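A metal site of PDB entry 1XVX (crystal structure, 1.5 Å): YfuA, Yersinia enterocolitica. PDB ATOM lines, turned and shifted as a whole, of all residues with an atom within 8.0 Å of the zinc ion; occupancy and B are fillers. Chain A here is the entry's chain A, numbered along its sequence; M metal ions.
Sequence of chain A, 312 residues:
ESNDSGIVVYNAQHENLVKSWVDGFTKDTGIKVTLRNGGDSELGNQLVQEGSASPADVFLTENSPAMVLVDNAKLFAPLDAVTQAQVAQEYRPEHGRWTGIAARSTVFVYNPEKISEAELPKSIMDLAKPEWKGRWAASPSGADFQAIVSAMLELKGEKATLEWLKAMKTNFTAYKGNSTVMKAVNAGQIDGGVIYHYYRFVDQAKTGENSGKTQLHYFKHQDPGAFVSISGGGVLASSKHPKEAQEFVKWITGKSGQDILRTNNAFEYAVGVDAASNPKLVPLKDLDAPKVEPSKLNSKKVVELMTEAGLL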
ATOM      1  N   SER A   2      11.451  16.542  25.467  1.00  0.00           N
ATOM      2  CA  SER A   2      12.774  16.300  24.798  1.00  0.00           C
ATOM      3  C   SER A   2      12.928  14.883  24.219  1.00  0.00           C
ATOM      4  O   SER A   2      13.442  14.728  23.115  1.00  0.00           O
ATOM      5  CB  SER A   2      13.938  16.622  25.733  1.00  0.00           C
ATOM      6  OG  SER A   2      15.179  16.338  25.121  1.00  0.00           O
ATOM      7  N   ASN A   3      12.529  13.868  24.979  1.00  0.00           N
ATOM      8  CA  ASN A   3      12.413  12.521  24.417  1.00  0.00           C
ATOM      9  C   ASN A   3      10.969  12.252  24.022  1.00  0.00           C
ATOM     10  O   ASN A   3      10.040  12.641  24.736  1.00  0.00           O
ATOM     11  CB  ASN A   3      12.858  11.437  25.407  1.00  0.00           C
ATOM     12  CG  ASN A   3      14.315  11.559  25.820  1.00  0.00           C
ATOM     13  OD1 ASN A   3      14.625  11.713  27.003  1.00  0.00           O
ATOM     14  ND2 ASN A   3      15.215  11.489  24.847  1.00  0.00           N
ATOM     15  N   ASP A   4      10.771  11.589  22.892  1.00  0.00           N
ATOM     16  CA  ASP A   4       9.430  11.211  22.485  1.00  0.00           C
ATOM     17  C   ASP A   4       9.043   9.868  23.121  1.00  0.00           C
ATOM     18  O   ASP A   4       9.650   9.460  24.115  1.00  0.00           O
ATOM     19  CB  ASP A   4       9.251  11.256  20.942  1.00  0.00           C
ATOM     20  CG  ASP A   4      10.149  10.270  20.192  1.00  0.00           C
ATOM     21  OD1 ASP A   4      10.648   9.282  20.775  1.00  0.00           O
ATOM     22  OD2 ASP A   4      10.346  10.481  18.982  1.00  0.00           O
ATOM     23  N   SER A   5       8.048   9.194  22.561  1.00  0.00           N
ATOM     24  CA  SER A   5       7.586   7.928  23.144  1.00  0.00           C
ATOM     25  C   SER A   5       8.555   6.772  22.892  1.00  0.00           C
ATOM     26  O   SER A   5       8.376   5.675  23.437  1.00  0.00           O
ATOM     27  CB  SER A   5       6.187   7.574  22.651  1.00  0.00           C
ATOM     28  OG  SER A   5       5.264   8.565  23.096  1.00  0.00           O
ATOM     29  N   GLY A   6       9.583   7.014  22.078  1.00  0.00           N
ATOM     30  CA  GLY A   6      10.622   6.031  21.833  1.00  0.00           C
ATOM     31  C   GLY A   6      10.311   5.016  20.755  1.00  0.00           C
ATOM     32  O   GLY A   6       9.471   5.250  19.880  1.00  0.00           O
ATOM     33  N   ILE A   7      11.002   3.887  20.820  1.00  0.00           N
ATOM     34  CA  ILE A   7      10.957   2.905  19.740  1.00  0.00           C
ATOM     35  C   ILE A   7      10.180   1.641  20.102  1.00  0.00           C
ATOM     36  O   ILE A   7       9.972   1.330  21.279  1.00  0.00           O
ATOM     37  CB  ILE A   7      12.385   2.536  19.244  1.00  0.00           C
ATOM     38  CG1 ILE A   7      13.218   1.922  20.379  1.00  0.00           C
ATOM     39  CG2 ILE A   7      13.090   3.758  18.696  1.00  0.00           C
ATOM     40  CD1 ILE A   7      14.565   1.347  19.927  1.00  0.00           C
ATOM     41  N   ILE A  31      16.014   7.127  25.729  1.00  0.00           N
ATOM     42  CA  ILE A  31      15.125   6.584  24.702  1.00  0.00           C
ATOM     43  C   ILE A  31      14.362   5.405  25.281  1.00  0.00           C
ATOM     44  O   ILE A  31      14.948   4.406  25.715  1.00  0.00           O
ATOM     45  CB  ILE A  31      15.917   6.182  23.437  1.00  0.00           C
ATOM     46  CG1 ILE A  31      16.620   7.413  22.840  1.00  0.00           C
ATOM     47  CG2 ILE A  31      14.989   5.506  22.401  1.00  0.00           C
ATOM     48  CD1 ILE A  31      17.734   7.069  21.813  1.00  0.00           C
ATOM     49  N   LYS A  32      13.031   5.541  25.290  1.00  0.00           N
ATOM     50  CA  LYS A  32      12.135   4.496  25.778  1.00  0.00           C
ATOM     51  C   LYS A  32      12.028   3.361  24.754  1.00  0.00           C
ATOM     52  O   LYS A  32      12.070   3.599  23.547  1.00  0.00           O
ATOM     53  CB  LYS A  32      10.759   5.071  26.092  1.00  0.00           C
ATOM     54  CG  LYS A  32      10.743   6.090  27.234  1.00  0.00           C
ATOM     55  CD  LYS A  32       9.314   6.565  27.516  1.00  0.00           C
ATOM     56  CE  LYS A  32       9.293   7.920  28.239  1.00  0.00           C
ATOM     57  NZ  LYS A  32       9.386   9.073  27.277  1.00  0.00           N
ATOM     58  N   ASP A  57      10.473  -0.516  14.728  1.00  0.00           N
ATOM     59  CA  ASP A  57      11.666   0.273  14.450  1.00  0.00           C
ATOM     60  C   ASP A  57      12.932  -0.589  14.332  1.00  0.00           C
ATOM     61  O   ASP A  57      13.810  -0.299  13.521  1.00  0.00           O
ATOM     62  CB  ASP A  57      11.815   1.333  15.525  1.00  0.00           C
ATOM     63  CG  ASP A  57      10.631   2.245  15.598  1.00  0.00           C
ATOM     64  OD1 ASP A  57      10.311   2.885  14.564  1.00  0.00           O
ATOM     65  OD2 ASP A  57      10.018   2.319  16.675  1.00  0.00           O
ATOM     66  N   SER A 239      10.762   2.690   9.663  1.00  0.00           N
ATOM     67  CA  SER A 239      10.779   3.322  10.991  1.00  0.00           C
ATOM     68  C   SER A 239      10.442   4.808  10.918  1.00  0.00           C
ATOM     69  O   SER A 239      11.017   5.530  10.102  1.00  0.00           O
ATOM     70  CB  SER A 239      12.149   3.176  11.638  1.00  0.00           C
ATOM     71  OG  SER A 239      12.180   3.816  12.891  1.00  0.00           O
ATOM     72  N   LYS A 240       9.525   5.240  11.791  1.00  0.00           N
ATOM     73  CA  LYS A 240       9.228   6.663  11.970  1.00  0.00           C
ATOM     74  C   LYS A 240      10.096   7.269  13.075  1.00  0.00           C
ATOM     75  O   LYS A 240       9.955   8.445  13.407  1.00  0.00           O
ATOM     76  CB  LYS A 240       7.735   6.856  12.280  1.00  0.00           C
ATOM     77  CG  LYS A 240       6.817   6.518  11.091  1.00  0.00           C
ATOM     78  CD  LYS A 240       5.332   6.739  11.424  1.00  0.00           C
ATOM     79  CE  LYS A 240       4.476   6.577  10.162  1.00  0.00           C
ATOM     80  NZ  LYS A 240       4.447   5.162   9.672  1.00  0.00           N
ATOM     81  N   HIS A 241      10.999   6.445  13.629  1.00  0.00           N
ATOM     82  CA  HIS A 241      11.965   6.861  14.649  1.00  0.00           C
ATOM     83  C   HIS A 241      13.374   6.397  14.239  1.00  0.00           C
ATOM     84  O   HIS A 241      14.053   5.715  15.018  1.00  0.00           O
ATOM     85  CB  HIS A 241      11.531   6.289  16.014  1.00  0.00           C
ATOM     86  CG  HIS A 241      10.156   6.700  16.418  1.00  0.00           C
ATOM     87  ND1 HIS A 241       9.897   7.794  17.218  1.00  0.00           N
ATOM     88  CD2 HIS A 241       8.945   6.164  16.112  1.00  0.00           C
ATOM     89  CE1 HIS A 241       8.592   7.924  17.386  1.00  0.00           C
ATOM     90  NE2 HIS A 241       7.992   6.943  16.732  1.00  0.00           N
ATOM     91  N   PRO A 242      13.827   6.753  13.026  1.00  0.00           N
ATOM     92  CA  PRO A 242      15.061   6.178  12.446  1.00  0.00           C
ATOM     93  C   PRO A 242      16.347   6.411  13.242  1.00  0.00           C
ATOM     94  O   PRO A 242      17.156   5.500  13.350  1.00  0.00           O
ATOM     95  CB  PRO A 242      15.170   6.842  11.075  1.00  0.00           C
ATOM     96  CG  PRO A 242      14.357   8.093  11.195  1.00  0.00           C
ATOM     97  CD  PRO A 242      13.214   7.714  12.082  1.00  0.00           C
ATOM     98  N   LYS A 243      16.532   7.610  13.785  1.00  0.00           N
ATOM     99  CA  LYS A 243      17.773   7.886  14.526  1.00  0.00           C
ATOM    100  C   LYS A 243      17.821   7.122  15.853  1.00  0.00           C
ATOM    101  O   LYS A 243      18.865   6.558  16.221  1.00  0.00           O
ATOM    102  CB  LYS A 243      17.999   9.388  14.717  1.00  0.00           C
ATOM    103  CG  LYS A 243      19.373   9.716  15.306  1.00  0.00           C
ATOM    104  CD  LYS A 243      19.458  11.130  15.812  1.00  0.00           C
ATOM    105  CE  LYS A 243      20.677  11.330  16.694  1.00  0.00           C
ATOM    106  NZ  LYS A 243      21.941  11.310  15.895  1.00  0.00           N
ATOM    107  N   GLU A 244      16.687   7.105  16.572  1.00  0.00           N
ATOM    108  CA  GLU A 244      16.599   6.362  17.843  1.00  0.00           C
ATOM    109  C   GLU A 244      16.774   4.870  17.602  1.00  0.00           C
ATOM    110  O   GLU A 244      17.443   4.178  18.372  1.00  0.00           O
ATOM    111  CB  GLU A 244      15.285   6.682  18.552  1.00  0.00           C
ATOM    112  CG  GLU A 244      15.243   8.130  19.054  1.00  0.00           C
ATOM    113  CD  GLU A 244      13.903   8.811  18.843  1.00  0.00           C
ATOM    114  OE1 GLU A 244      12.890   8.094  18.677  1.00  0.00           O
ATOM    115  OE2 GLU A 244      13.857  10.053  18.867  1.00  0.00           O
ATOM    116  N   ALA A 245      16.186   4.380  16.515  1.00  0.00           N
ATOM    117  CA  ALA A 245      16.376   2.993  16.088  1.00  0.00           C
ATOM    118  C   ALA A 245      17.878   2.689  15.822  1.00  0.00           C
ATOM    119  O   ALA A 245      18.412   1.721  16.347  1.00  0.00           O
ATOM    120  CB  ALA A 245      15.516   2.677  14.856  1.00  0.00           C
HETATM  121 ZN    ZN M   1      11.283   9.117  17.927  1.00  0.00          ZN
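OD2 of Asp 4 binds the zinc ion.
The zinc ion is bound by ND1 of His 241, 2.0 Å away.
The side-chain carboxylate (OE1) of Glu 244 is bound to the zinc ion, 2.0 Å away.
The zinc ion has three donor atoms within binding distance.
Three residues have an atom within 4 Å of the zinc ion: Asp 4, His 241 and Glu 244.
The nearest printed residue that does not touch the zinc ion is Gly 6 (4.7 Å).
The side-chain carboxylate (OD1) of Asp 4 sits at hydrogen-bond distance from the backbone NH (N) of Gly 6.
The backbone carbonyl oxygen of Asp 4 sits at hydrogen-bond distance from the side-chain amino group of Lys 32.
N of His 241 lies within hydrogen-bond range of OG of Ser 239, 3.0 Å away.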
